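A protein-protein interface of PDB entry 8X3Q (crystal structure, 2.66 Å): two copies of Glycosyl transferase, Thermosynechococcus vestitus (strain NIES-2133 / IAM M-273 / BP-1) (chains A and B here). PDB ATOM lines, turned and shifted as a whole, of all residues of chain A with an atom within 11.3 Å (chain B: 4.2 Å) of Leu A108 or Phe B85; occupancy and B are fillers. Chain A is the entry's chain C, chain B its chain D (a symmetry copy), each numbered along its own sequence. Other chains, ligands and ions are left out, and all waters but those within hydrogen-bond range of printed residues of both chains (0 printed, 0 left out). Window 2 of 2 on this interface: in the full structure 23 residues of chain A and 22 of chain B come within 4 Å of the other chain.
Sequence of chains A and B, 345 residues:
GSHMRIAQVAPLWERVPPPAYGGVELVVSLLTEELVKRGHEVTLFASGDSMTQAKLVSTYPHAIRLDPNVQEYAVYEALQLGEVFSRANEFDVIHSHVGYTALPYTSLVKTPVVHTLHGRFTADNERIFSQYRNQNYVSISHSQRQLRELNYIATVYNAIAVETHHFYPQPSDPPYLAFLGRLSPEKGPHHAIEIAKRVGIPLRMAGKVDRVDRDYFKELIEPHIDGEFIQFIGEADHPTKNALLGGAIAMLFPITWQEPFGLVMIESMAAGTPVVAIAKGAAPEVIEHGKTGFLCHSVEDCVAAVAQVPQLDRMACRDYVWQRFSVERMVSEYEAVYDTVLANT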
ATOM      1  N   LEU A  81     -14.784 -25.351  14.150  1.00  0.00           N
ATOM      2  CA  LEU A  81     -15.144 -24.429  13.079  1.00  0.00           C
ATOM      3  C   LEU A  81     -16.656 -24.286  12.963  1.00  0.00           C
ATOM      4  O   LEU A  81     -17.161 -23.196  12.673  1.00  0.00           O
ATOM      5  CB  LEU A  81     -14.540 -24.893  11.756  1.00  0.00           C
ATOM      6  CG  LEU A  81     -13.110 -24.414  11.503  1.00  0.00           C
ATOM      7  CD1 LEU A  81     -12.488 -25.155  10.330  1.00  0.00           C
ATOM      8  CD2 LEU A  81     -13.095 -22.912  11.270  1.00  0.00           C
ATOM      9  N   GLY A  82     -17.391 -25.377  13.177  1.00  0.00           N
ATOM     10  CA  GLY A  82     -18.841 -25.281  13.194  1.00  0.00           C
ATOM     11  C   GLY A  82     -19.365 -24.507  14.387  1.00  0.00           C
ATOM     12  O   GLY A  82     -20.337 -23.757  14.270  1.00  0.00           O
ATOM     13  N   VAL A  84     -17.798 -22.029  15.971  1.00  0.00           N
ATOM     14  CA  VAL A  84     -17.456 -20.611  15.856  1.00  0.00           C
ATOM     15  C   VAL A  84     -18.453 -19.873  14.969  1.00  0.00           C
ATOM     16  O   VAL A  84     -19.114 -18.922  15.404  1.00  0.00           O
ATOM     17  CB  VAL A  84     -16.021 -20.445  15.328  1.00  0.00           C
ATOM     18  CG1 VAL A  84     -15.773 -18.999  14.925  1.00  0.00           C
ATOM     19  CG2 VAL A  84     -15.020 -20.888  16.367  1.00  0.00           C
ATOM     20  N   PHE A  85     -18.573 -20.301  13.711  1.00  0.00           N
ATOM     21  CA  PHE A  85     -19.346 -19.534  12.743  1.00  0.00           C
ATOM     22  C   PHE A  85     -20.846 -19.715  12.900  1.00  0.00           C
ATOM     23  O   PHE A  85     -21.610 -18.894  12.390  1.00  0.00           O
ATOM     24  CB  PHE A  85     -18.934 -19.924  11.324  1.00  0.00           C
ATOM     25  CG  PHE A  85     -17.564 -19.471  10.960  1.00  0.00           C
ATOM     26  CD1 PHE A  85     -16.459 -20.230  11.302  1.00  0.00           C
ATOM     27  CD2 PHE A  85     -17.377 -18.271  10.303  1.00  0.00           C
ATOM     28  CE1 PHE A  85     -15.190 -19.805  10.980  1.00  0.00           C
ATOM     29  CE2 PHE A  85     -16.114 -17.839   9.977  1.00  0.00           C
ATOM     30  CZ  PHE A  85     -15.016 -18.606  10.315  1.00  0.00           C
ATOM     31  N   SER A  86     -21.282 -20.763  13.593  1.00  0.00           N
ATOM     32  CA  SER A  86     -22.671 -20.876  14.010  1.00  0.00           C
ATOM     33  C   SER A  86     -22.989 -19.997  15.214  1.00  0.00           C
ATOM     34  O   SER A  86     -24.165 -19.870  15.569  1.00  0.00           O
ATOM     35  CB  SER A  86     -23.064 -22.331  14.263  1.00  0.00           C
ATOM     36  OG  SER A  86     -22.296 -22.950  15.288  1.00  0.00           O
ATOM     37  N   ARG A  87     -21.974 -19.466  15.906  1.00  0.00           N
ATOM     38  CA  ARG A  87     -22.191 -18.477  16.955  1.00  0.00           C
ATOM     39  C   ARG A  87     -21.755 -17.094  16.504  1.00  0.00           C
ATOM     40  O   ARG A  87     -21.464 -16.240  17.343  1.00  0.00           O
ATOM     41  CB  ARG A  87     -21.438 -18.828  18.236  1.00  0.00           C
ATOM     42  CG  ARG A  87     -21.817 -20.128  18.919  1.00  0.00           C
ATOM     43  CD  ARG A  87     -21.077 -20.239  20.269  1.00  0.00           C
ATOM     44  NE  ARG A  87     -21.181 -21.587  20.819  1.00  0.00           N
ATOM     45  CZ  ARG A  87     -20.732 -21.941  22.024  1.00  0.00           C
ATOM     46  NH1 ARG A  87     -20.304 -21.013  22.876  1.00  0.00           N
ATOM     47  NH2 ARG A  87     -20.818 -23.212  22.429  1.00  0.00           N
ATOM     48  N   ALA A  88     -21.672 -16.879  15.189  1.00  0.00           N
ATOM     49  CA  ALA A  88     -21.074 -15.656  14.663  1.00  0.00           C
ATOM     50  C   ALA A  88     -21.754 -14.391  15.170  1.00  0.00           C
ATOM     51  O   ALA A  88     -21.095 -13.357  15.313  1.00  0.00           O
ATOM     52  CB  ALA A  88     -21.083 -15.684  13.136  1.00  0.00           C
ATOM     53  N   ASN A  89     -23.056 -14.446  15.450  1.00  0.00           N
ATOM     54  CA  ASN A  89     -23.751 -13.259  15.933  1.00  0.00           C
ATOM     55  C   ASN A  89     -23.365 -12.872  17.356  1.00  0.00           C
ATOM     56  O   ASN A  89     -23.735 -11.780  17.799  1.00  0.00           O
ATOM     57  CB  ASN A  89     -25.263 -13.447  15.830  1.00  0.00           C
ATOM     58  CG  ASN A  89     -25.850 -12.732  14.629  1.00  0.00           C
ATOM     59  OD1 ASN A  89     -25.488 -11.590  14.337  1.00  0.00           O
ATOM     60  ND2 ASN A  89     -26.765 -13.393  13.932  1.00  0.00           N
ATOM     61  N   ILE A  94     -14.253 -12.068  14.376  1.00  0.00           N
ATOM     62  CA  ILE A  94     -13.666 -13.387  14.579  1.00  0.00           C
ATOM     63  C   ILE A  94     -12.203 -13.326  14.164  1.00  0.00           C
ATOM     64  O   ILE A  94     -11.884 -12.933  13.036  1.00  0.00           O
ATOM     65  CB  ILE A  94     -14.420 -14.466  13.786  1.00  0.00           C
ATOM     66  CG1 ILE A  94     -15.894 -14.496  14.192  1.00  0.00           C
ATOM     67  CG2 ILE A  94     -13.774 -15.829  13.993  1.00  0.00           C
ATOM     68  CD1 ILE A  94     -16.736 -15.447  13.371  1.00  0.00           C
ATOM     69  N   THR A 101      -8.644 -23.422   6.429  1.00  0.00           N
ATOM     70  CA  THR A 101      -9.860 -24.180   6.707  1.00  0.00           C
ATOM     71  C   THR A 101     -11.031 -23.284   7.095  1.00  0.00           C
ATOM     72  O   THR A 101     -12.179 -23.744   7.082  1.00  0.00           O
ATOM     73  CB  THR A 101      -9.605 -25.203   7.818  1.00  0.00           C
ATOM     74  OG1 THR A 101      -8.831 -24.599   8.860  1.00  0.00           O
ATOM     75  CG2 THR A 101      -8.858 -26.411   7.270  1.00  0.00           C
ATOM     76  N   ALA A 102     -10.772 -22.021   7.436  1.00  0.00           N
ATOM     77  CA  ALA A 102     -11.820 -21.085   7.817  1.00  0.00           C
ATOM     78  C   ALA A 102     -12.284 -20.196   6.669  1.00  0.00           C
ATOM     79  O   ALA A 102     -13.302 -19.511   6.816  1.00  0.00           O
ATOM     80  CB  ALA A 102     -11.347 -20.203   8.980  1.00  0.00           C
ATOM     81  N   LEU A 103     -11.564 -20.178   5.546  1.00  0.00           N
ATOM     82  CA  LEU A 103     -11.948 -19.309   4.433  1.00  0.00           C
ATOM     83  C   LEU A 103     -13.333 -19.620   3.876  1.00  0.00           C
ATOM     84  O   LEU A 103     -14.130 -18.679   3.718  1.00  0.00           O
ATOM     85  CB  LEU A 103     -10.885 -19.370   3.329  1.00  0.00           C
ATOM     86  CG  LEU A 103      -9.414 -19.180   3.697  1.00  0.00           C
ATOM     87  CD1 LEU A 103      -8.586 -19.015   2.433  1.00  0.00           C
ATOM     88  CD2 LEU A 103      -9.228 -17.992   4.625  1.00  0.00           C
ATOM     89  N   PRO A 104     -13.691 -20.869   3.550  1.00  0.00           N
ATOM     90  CA  PRO A 104     -15.036 -21.109   2.996  1.00  0.00           C
ATOM     91  C   PRO A 104     -16.170 -20.795   3.960  1.00  0.00           C
ATOM     92  O   PRO A 104     -17.300 -20.577   3.507  1.00  0.00           O
ATOM     93  CB  PRO A 104     -15.011 -22.599   2.624  1.00  0.00           C
ATOM     94  CG  PRO A 104     -13.863 -23.175   3.365  1.00  0.00           C
ATOM     95  CD  PRO A 104     -12.867 -22.092   3.534  1.00  0.00           C
ATOM     96  N   TYR A 105     -15.914 -20.772   5.270  1.00  0.00           N
ATOM     97  CA  TYR A 105     -16.944 -20.389   6.228  1.00  0.00           C
ATOM     98  C   TYR A 105     -17.147 -18.882   6.300  1.00  0.00           C
ATOM     99  O   TYR A 105     -18.230 -18.433   6.692  1.00  0.00           O
ATOM    100  CB  TYR A 105     -16.599 -20.912   7.625  1.00  0.00           C
ATOM    101  CG  TYR A 105     -16.579 -22.417   7.741  1.00  0.00           C
ATOM    102  CD1 TYR A 105     -15.420 -23.136   7.481  1.00  0.00           C
ATOM    103  CD2 TYR A 105     -17.715 -23.120   8.121  1.00  0.00           C
ATOM    104  CE1 TYR A 105     -15.394 -24.509   7.589  1.00  0.00           C
ATOM    105  CE2 TYR A 105     -17.699 -24.496   8.230  1.00  0.00           C
ATOM    106  CZ  TYR A 105     -16.535 -25.185   7.963  1.00  0.00           C
ATOM    107  OH  TYR A 105     -16.504 -26.554   8.068  1.00  0.00           O
ATOM    108  N   THR A 106     -16.131 -18.098   5.926  1.00  0.00           N
ATOM    109  CA  THR A 106     -16.174 -16.655   6.145  1.00  0.00           C
ATOM    110  C   THR A 106     -17.224 -15.986   5.262  1.00  0.00           C
ATOM    111  O   THR A 106     -17.889 -15.035   5.690  1.00  0.00           O
ATOM    112  CB  THR A 106     -14.787 -16.058   5.899  1.00  0.00           C
ATOM    113  OG1 THR A 106     -13.854 -16.625   6.831  1.00  0.00           O
ATOM    114  CG2 THR A 106     -14.803 -14.550   6.073  1.00  0.00           C
ATOM    115  N   SER A 107     -17.396 -16.472   4.029  1.00  0.00           N
ATOM    116  CA  SER A 107     -18.395 -15.905   3.131  1.00  0.00           C
ATOM    117  C   SER A 107     -19.820 -16.268   3.528  1.00  0.00           C
ATOM    118  O   SER A 107     -20.763 -15.736   2.933  1.00  0.00           O
ATOM    119  CB  SER A 107     -18.136 -16.359   1.691  1.00  0.00           C
ATOM    120  OG  SER A 107     -18.533 -17.706   1.501  1.00  0.00           O
ATOM    121  N   LEU A 108     -19.998 -17.154   4.507  1.00  0.00           N
ATOM    122  CA  LEU A 108     -21.316 -17.631   4.900  1.00  0.00           C
ATOM    123  C   LEU A 108     -21.887 -16.908   6.113  1.00  0.00           C
ATOM    124  O   LEU A 108     -23.046 -17.155   6.468  1.00  0.00           O
ATOM    125  CB  LEU A 108     -21.265 -19.139   5.187  1.00  0.00           C
ATOM    126  CG  LEU A 108     -21.114 -20.055   3.969  1.00  0.00           C
ATOM    127  CD1 LEU A 108     -21.059 -21.515   4.393  1.00  0.00           C
ATOM    128  CD2 LEU A 108     -22.241 -19.825   2.973  1.00  0.00           C
ATOM    129  N   VAL A 109     -21.118 -16.029   6.756  1.00  0.00           N
ATOM    130  CA  VAL A 109     -21.554 -15.356   7.973  1.00  0.00           C
ATOM    131  C   VAL A 109     -21.422 -13.849   7.794  1.00  0.00           C
ATOM    132  O   VAL A 109     -20.621 -13.366   6.989  1.00  0.00           O
ATOM    133  CB  VAL A 109     -20.755 -15.825   9.210  1.00  0.00           C
ATOM    134  CG1 VAL A 109     -20.851 -17.334   9.368  1.00  0.00           C
ATOM    135  CG2 VAL A 109     -19.302 -15.385   9.104  1.00  0.00           C
ATOM    136  N   LYS A 110     -22.232 -13.107   8.555  1.00  0.00           N
ATOM    137  CA  LYS A 110     -22.164 -11.649   8.517  1.00  0.00           C
ATOM    138  C   LYS A 110     -20.926 -11.130   9.240  1.00  0.00           C
ATOM    139  O   LYS A 110     -20.283 -10.180   8.782  1.00  0.00           O
ATOM    140  CB  LYS A 110     -23.419 -11.042   9.144  1.00  0.00           C
ATOM    141  CG  LYS A 110     -24.739 -11.623   8.665  1.00  0.00           C
ATOM    142  CD  LYS A 110     -25.779 -11.555   9.780  1.00  0.00           C
ATOM    143  CE  LYS A 110     -27.175 -11.897   9.285  1.00  0.00           C
ATOM    144  NZ  LYS A 110     -27.979 -10.675   9.003  1.00  0.00           N
ATOM    145  N   THR A 111     -20.590 -11.738  10.373  1.00  0.00           N
ATOM    146  CA  THR A 111     -19.525 -11.227  11.226  1.00  0.00           C
ATOM    147  C   THR A 111     -18.190 -11.240  10.486  1.00  0.00           C
ATOM    148  O   THR A 111     -17.803 -12.280   9.935  1.00  0.00           O
ATOM    149  CB  THR A 111     -19.425 -12.061  12.503  1.00  0.00           C
ATOM    150  OG1 THR A 111     -20.687 -12.046  13.183  1.00  0.00           O
ATOM    151  CG2 THR A 111     -18.352 -11.503  13.425  1.00  0.00           C
ATOM    152  N   PRO A 112     -17.467 -10.123  10.448  1.00  0.00           N
ATOM    153  CA  PRO A 112     -16.178 -10.106   9.749  1.00  0.00           C
ATOM    154  C   PRO A 112     -15.155 -10.981  10.454  1.00  0.00           C
ATOM    155  O   PRO A 112     -15.150 -11.111  11.681  1.00  0.00           O
ATOM    156  CB  PRO A 112     -15.771  -8.628   9.790  1.00  0.00           C
ATOM    157  CG  PRO A 112     -16.508  -8.070  10.967  1.00  0.00           C
ATOM    158  CD  PRO A 112     -17.812  -8.805  11.007  1.00  0.00           C
ATOM    159  N   VAL A 113     -14.277 -11.582   9.656  1.00  0.00           N
ATOM    160  CA  VAL A 113     -13.282 -12.533  10.137  1.00  0.00           C
ATOM    161  C   VAL A 113     -11.895 -12.007   9.794  1.00  0.00           C
ATOM    162  O   VAL A 113     -11.663 -11.540   8.673  1.00  0.00           O
ATOM    163  CB  VAL A 113     -13.501 -13.931   9.529  1.00  0.00           C
ATOM    164  CG1 VAL A 113     -12.471 -14.915  10.062  1.00  0.00           C
ATOM    165  CG2 VAL A 113     -14.912 -14.419   9.816  1.00  0.00           C
ATOM    166  N   HIS A 115      -7.913 -13.150   9.576  1.00  0.00           N
ATOM    167  CA  HIS A 115      -7.057 -14.325   9.440  1.00  0.00           C
ATOM    168  C   HIS A 115      -5.609 -13.900   9.662  1.00  0.00           C
ATOM    169  O   HIS A 115      -5.039 -13.174   8.840  1.00  0.00           O
ATOM    170  CB  HIS A 115      -7.216 -14.975   8.066  1.00  0.00           C
ATOM    171  CG  HIS A 115      -8.630 -15.317   7.711  1.00  0.00           C
ATOM    172  ND1 HIS A 115      -9.262 -16.452   8.172  1.00  0.00           N
ATOM    173  CD2 HIS A 115      -9.528 -14.680   6.924  1.00  0.00           C
ATOM    174  CE1 HIS A 115     -10.491 -16.495   7.691  1.00  0.00           C
ATOM    175  NE2 HIS A 115     -10.679 -15.431   6.931  1.00  0.00           N
ATOM    176  N   TYR A 132     -10.032 -16.496  -2.171  1.00  0.00           N
ATOM    177  CA  TYR A 132     -10.502 -15.646  -1.086  1.00  0.00           C
ATOM    178  C   TYR A 132      -9.532 -14.492  -0.870  1.00  0.00           C
ATOM    179  O   TYR A 132      -9.173 -14.151   0.260  1.00  0.00           O
ATOM    180  CB  TYR A 132     -10.701 -16.458   0.190  1.00  0.00           C
ATOM    181  CG  TYR A 132     -11.736 -17.550   0.037  1.00  0.00           C
ATOM    182  CD1 TYR A 132     -13.093 -17.256   0.077  1.00  0.00           C
ATOM    183  CD2 TYR A 132     -11.357 -18.870  -0.167  1.00  0.00           C
ATOM    184  CE1 TYR A 132     -14.045 -18.250  -0.068  1.00  0.00           C
ATOM    185  CE2 TYR A 132     -12.302 -19.870  -0.315  1.00  0.00           C
ATOM    186  CZ  TYR A 132     -13.643 -19.555  -0.264  1.00  0.00           C
ATOM    187  OH  TYR A 132     -14.587 -20.548  -0.411  1.00  0.00           O
ATOM    188  N   GLN A 135     -10.272 -11.109   1.470  1.00  0.00           N
ATOM    189  CA  GLN A 135     -10.529 -11.288   2.889  1.00  0.00           C
ATOM    190  C   GLN A 135      -9.422 -10.632   3.702  1.00  0.00           C
ATOM    191  O   GLN A 135      -8.362 -10.271   3.185  1.00  0.00           O
ATOM    192  CB  GLN A 135     -10.653 -12.777   3.234  1.00  0.00           C
ATOM    193  CG  GLN A 135     -11.754 -13.486   2.465  1.00  0.00           C
ATOM    194  CD  GLN A 135     -12.292 -14.696   3.196  1.00  0.00           C
ATOM    195  OE1 GLN A 135     -13.458 -15.061   3.041  1.00  0.00           O
ATOM    196  NE2 GLN A 135     -11.445 -15.329   3.999  1.00  0.00           N
ATOM    197  N   LEU B  81     -15.980 -27.460  -1.169  1.00  0.00           N
ATOM    198  CA  LEU B  81     -17.002 -27.258  -0.146  1.00  0.00           C
ATOM    199  C   LEU B  81     -17.453 -25.803  -0.109  1.00  0.00           C
ATOM    200  O   LEU B  81     -18.636 -25.518   0.099  1.00  0.00           O
ATOM    201  CB  LEU B  81     -16.481 -27.701   1.222  1.00  0.00           C
ATOM    202  CG  LEU B  81     -16.368 -29.214   1.430  1.00  0.00           C
ATOM    203  CD1 LEU B  81     -15.685 -29.533   2.752  1.00  0.00           C
ATOM    204  CD2 LEU B  81     -17.739 -29.873   1.352  1.00  0.00           C
ATOM    205  N   GLY B  82     -16.525 -24.870  -0.322  1.00  0.00           N
ATOM    206  CA  GLY B  82     -16.912 -23.477  -0.442  1.00  0.00           C
ATOM    207  C   GLY B  82     -17.717 -23.211  -1.699  1.00  0.00           C
ATOM    208  O   GLY B  82     -18.631 -22.382  -1.700  1.00  0.00           O
ATOM    209  N   GLU B  83     -17.394 -23.917  -2.787  1.00  0.00           N
ATOM    210  CA  GLU B  83     -18.133 -23.747  -4.036  1.00  0.00           C
ATOM    211  C   GLU B  83     -19.580 -24.202  -3.893  1.00  0.00           C
ATOM    212  O   GLU B  83     -20.497 -23.540  -4.395  1.00  0.00           O
ATOM    213  CB  GLU B  83     -17.442 -24.518  -5.161  1.00  0.00           C
ATOM    214  CG  GLU B  83     -16.456 -23.700  -5.974  1.00  0.00           C
ATOM    215  CD  GLU B  83     -17.045 -22.391  -6.459  1.00  0.00           C
ATOM    216  OE1 GLU B  83     -17.835 -22.415  -7.423  1.00  0.00           O
ATOM    217  OE2 GLU B  83     -16.714 -21.335  -5.884  1.00  0.00           O
ATOM    218  N   VAL B  84     -19.803 -25.332  -3.220  1.00  0.00           N
ATOM    219  CA  VAL B  84     -21.152 -25.881  -3.094  1.00  0.00           C
ATOM    220  C   VAL B  84     -22.048 -24.916  -2.327  1.00  0.00           C
ATOM    221  O   VAL B  84     -23.095 -24.480  -2.821  1.00  0.00           O
ATOM    222  CB  VAL B  84     -21.113 -27.263  -2.418  1.00  0.00           C
ATOM    223  CG1 VAL B  84     -22.524 -27.742  -2.106  1.00  0.00           C
ATOM    224  CG2 VAL B  84     -20.386 -28.265  -3.300  1.00  0.00           C
ATOM    225  N   PHE B  85     -21.649 -24.573  -1.102  1.00  0.00           N
ATOM    226  CA  PHE B  85     -22.501 -23.795  -0.214  1.00  0.00           C
ATOM    227  C   PHE B  85     -22.504 -22.304  -0.526  1.00  0.00           C
ATOM    228  O   PHE B  85     -23.387 -21.593  -0.034  1.00  0.00           O
ATOM    229  CB  PHE B  85     -22.092 -24.042   1.238  1.00  0.00           C
ATOM    230  CG  PHE B  85     -22.179 -25.487   1.639  1.00  0.00           C
ATOM    231  CD1 PHE B  85     -23.388 -26.042   2.017  1.00  0.00           C
ATOM    232  CD2 PHE B  85     -21.058 -26.297   1.608  1.00  0.00           C
ATOM    233  CE1 PHE B  85     -23.474 -27.374   2.372  1.00  0.00           C
ATOM    234  CE2 PHE B  85     -21.136 -27.630   1.958  1.00  0.00           C
ATOM    235  CZ  PHE B  85     -22.345 -28.170   2.342  1.00  0.00           C
ATOM    236  N   SER B  86     -21.556 -21.804  -1.323  1.00  0.00           N
ATOM    237  CA  SER B  86     -21.711 -20.451  -1.840  1.00  0.00           C
ATOM    238  C   SER B  86     -22.731 -20.391  -2.965  1.00  0.00           C
ATOM    239  O   SER B  86     -23.270 -19.314  -3.243  1.00  0.00           O
ATOM    240  CB  SER B  86     -20.370 -19.905  -2.336  1.00  0.00           C
ATOM    241  OG  SER B  86     -19.924 -20.617  -3.479  1.00  0.00           O
ATOM    242  N   ARG B  87     -23.009 -21.524  -3.611  1.00  0.00           N
ATOM    243  CA  ARG B  87     -24.099 -21.643  -4.569  1.00  0.00           C
ATOM    244  C   ARG B  87     -25.208 -22.553  -4.055  1.00  0.00           C
ATOM    245  O   ARG B  87     -26.010 -23.053  -4.847  1.00  0.00           O
ATOM    246  CB  ARG B  87     -23.580 -22.130  -5.920  1.00  0.00           C
ATOM    247  CG  ARG B  87     -22.636 -21.148  -6.587  1.00  0.00           C
ATOM    248  CD  ARG B  87     -22.102 -21.718  -7.878  1.00  0.00           C
ATOM    249  NE  ARG B  87     -21.056 -22.689  -7.602  1.00  0.00           N
ATOM    250  CZ  ARG B  87     -20.386 -23.356  -8.532  1.00  0.00           C
ATOM    251  NH1 ARG B  87     -20.638 -23.155  -9.818  1.00  0.00           N
ATOM    252  NH2 ARG B  87     -19.452 -24.215  -8.163  1.00  0.00           N
ATOM    253  N   ALA B  88     -25.251 -22.788  -2.738  1.00  0.00           N
ATOM    254  CA  ALA B  88     -26.263 -23.668  -2.160  1.00  0.00           C
ATOM    255  C   ALA B  88     -27.663 -23.187  -2.501  1.00  0.00           C
ATOM    256  O   ALA B  88     -28.606 -23.986  -2.560  1.00  0.00           O
ATOM    257  CB  ALA B  88     -26.086 -23.757  -0.645  1.00  0.00           C
ATOM    258  N   TYR B 105     -21.206 -27.109   7.632  1.00  0.00           N
ATOM    259  CA  TYR B 105     -21.794 -26.243   6.618  1.00  0.00           C
ATOM    260  C   TYR B 105     -23.312 -26.347   6.557  1.00  0.00           C
ATOM    261  O   TYR B 105     -23.965 -25.400   6.102  1.00  0.00           O
ATOM    262  CB  TYR B 105     -21.227 -26.575   5.238  1.00  0.00           C
ATOM    263  CG  TYR B 105     -19.774 -26.222   5.051  1.00  0.00           C
ATOM    264  CD1 TYR B 105     -19.393 -24.941   4.675  1.00  0.00           C
ATOM    265  CD2 TYR B 105     -18.780 -27.174   5.238  1.00  0.00           C
ATOM    266  CE1 TYR B 105     -18.064 -24.616   4.497  1.00  0.00           C
ATOM    267  CE2 TYR B 105     -17.450 -26.859   5.063  1.00  0.00           C
ATOM    268  CZ  TYR B 105     -17.098 -25.580   4.693  1.00  0.00           C
ATOM    269  OH  TYR B 105     -15.774 -25.266   4.519  1.00  0.00           O
ATOM    270  N   LEU B 108     -25.588 -23.726   8.199  1.00  0.00           N
ATOM    271  CA  LEU B 108     -25.408 -22.351   7.751  1.00  0.00           C
ATOM    272  C   LEU B 108     -26.230 -21.988   6.519  1.00  0.00           C
ATOM    273  O   LEU B 108     -26.270 -20.809   6.153  1.00  0.00           O
ATOM    274  CB  LEU B 108     -23.928 -22.087   7.447  1.00  0.00           C
ATOM    275  CG  LEU B 108     -22.943 -22.122   8.617  1.00  0.00           C
ATOM    276  CD1 LEU B 108     -21.518 -21.939   8.114  1.00  0.00           C
ATOM    277  CD2 LEU B 108     -23.294 -21.055   9.643  1.00  0.00           C
ATOM    278  N   VAL B 109     -26.888 -22.954   5.875  1.00  0.00           N
ATOM    279  CA  VAL B 109     -27.609 -22.701   4.636  1.00  0.00           C
ATOM    280  C   VAL B 109     -29.042 -23.199   4.765  1.00  0.00           C
ATOM    281  O   VAL B 109     -29.356 -24.076   5.574  1.00  0.00           O
ATOM    282  CB  VAL B 109     -26.923 -23.349   3.413  1.00  0.00           C
ATOM    283  CG1 VAL B 109     -25.511 -22.805   3.243  1.00  0.00           C
ATOM    284  CG2 VAL B 109     -26.903 -24.863   3.547  1.00  0.00           C
ATOM    285  N   VAL B 113     -29.401 -30.745   3.136  1.00  0.00           N
ATOM    286  CA  VAL B 113     -28.274 -31.553   2.688  1.00  0.00           C
ATOM    287  C   VAL B 113     -28.510 -32.991   3.126  1.00  0.00           C
ATOM    288  O   VAL B 113     -28.886 -33.240   4.278  1.00  0.00           O
ATOM    289  CB  VAL B 113     -26.940 -31.026   3.248  1.00  0.00           C
ATOM    290  CG1 VAL B 113     -25.783 -31.903   2.788  1.00  0.00           C
ATOM    291  CG2 VAL B 113     -26.722 -29.580   2.831  1.00  0.00           C
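O of Gly B82 is in hydrogen-bond range of OG of Ser B86 (2.8 Å).
Phe A85 touches Leu B108 (O to CD2, 3.9 Å).
CB of Pro A104 touches CA of Gly B82 (3.7 Å).
Tyr B105 touches Pro A104.
Tyr B105 touches Tyr A105 (CE2 to OH, 3.2 Å).
Leu B108 touches Tyr A105.
CD2 of Leu A108 touches O of Phe B85 (3.7 Å).
Leu A108 touches Tyr B105.
CD1 of Leu A108 touches CD1 of Leu B108, 3.8 Å away.
Gly B82 touches Tyr A132.
Of the printed residues of chain B, Pro A104 touches Gly B82 (3.7 Å) and Tyr B105 (3.1 Å).
Of the printed residues of chain B, Tyr A105 touches Tyr B105 and Leu B108.
Leu A108 touches three residues of chain B.
Of the printed residues of chain B, Tyr A132 touches Gly B82.
No residue of chain A comes within 4 Å of Leu B81.
Of the printed residues of chain A, Gly B82 touches Pro A104 and Tyr A132.
No residue of chain A comes within 4 Å of Val B84.
Of chain A, only Leu A108 (3.7 Å) comes within 4 Å of Phe B85.
No residue of chain A comes within 4 Å of Ser B86.
The nearest printed residue of chain B that does not touch Phe A85 is Tyr B105 (8.3 Å).
Hydrophobic or aromatic side chains of chain A within 4 Å of the printed part of chain B: Pro A104, Tyr A105, Leu A108 and Tyr A132.
Along chain A the printed residues that touch a printed residue of chain B span positions 85 to 132.
Of the 12 printed residues of chain B, 4 touch a printed residue of chain A.
Printed residues of chain B that touch a printed residue of chain A: Gly B82, Phe B85, Tyr B105 and Leu B108.
Hydrophobic or aromatic side chains of chain B that line the printed part of chain A: Tyr B105 and Leu B108.
Phe A85 touches Leu B108, and with the chains exchanged Leu A108 touches Phe B85.
Tyr A105 touches its own counterpart, Tyr B105.
Tyr A105 touches Leu B108, and with the chains exchanged Leu A108 touches Tyr B105.
Leu B108 touches its own counterpart, Leu A108.
Positions printed for both chains: 81, 82, 84, 85, 86, 87, 88, 105, 108, 109 and 113.
Of the 9 pairs that touch across the chains among the printed residues, 6 have their exchanged pair printed and touching as well.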
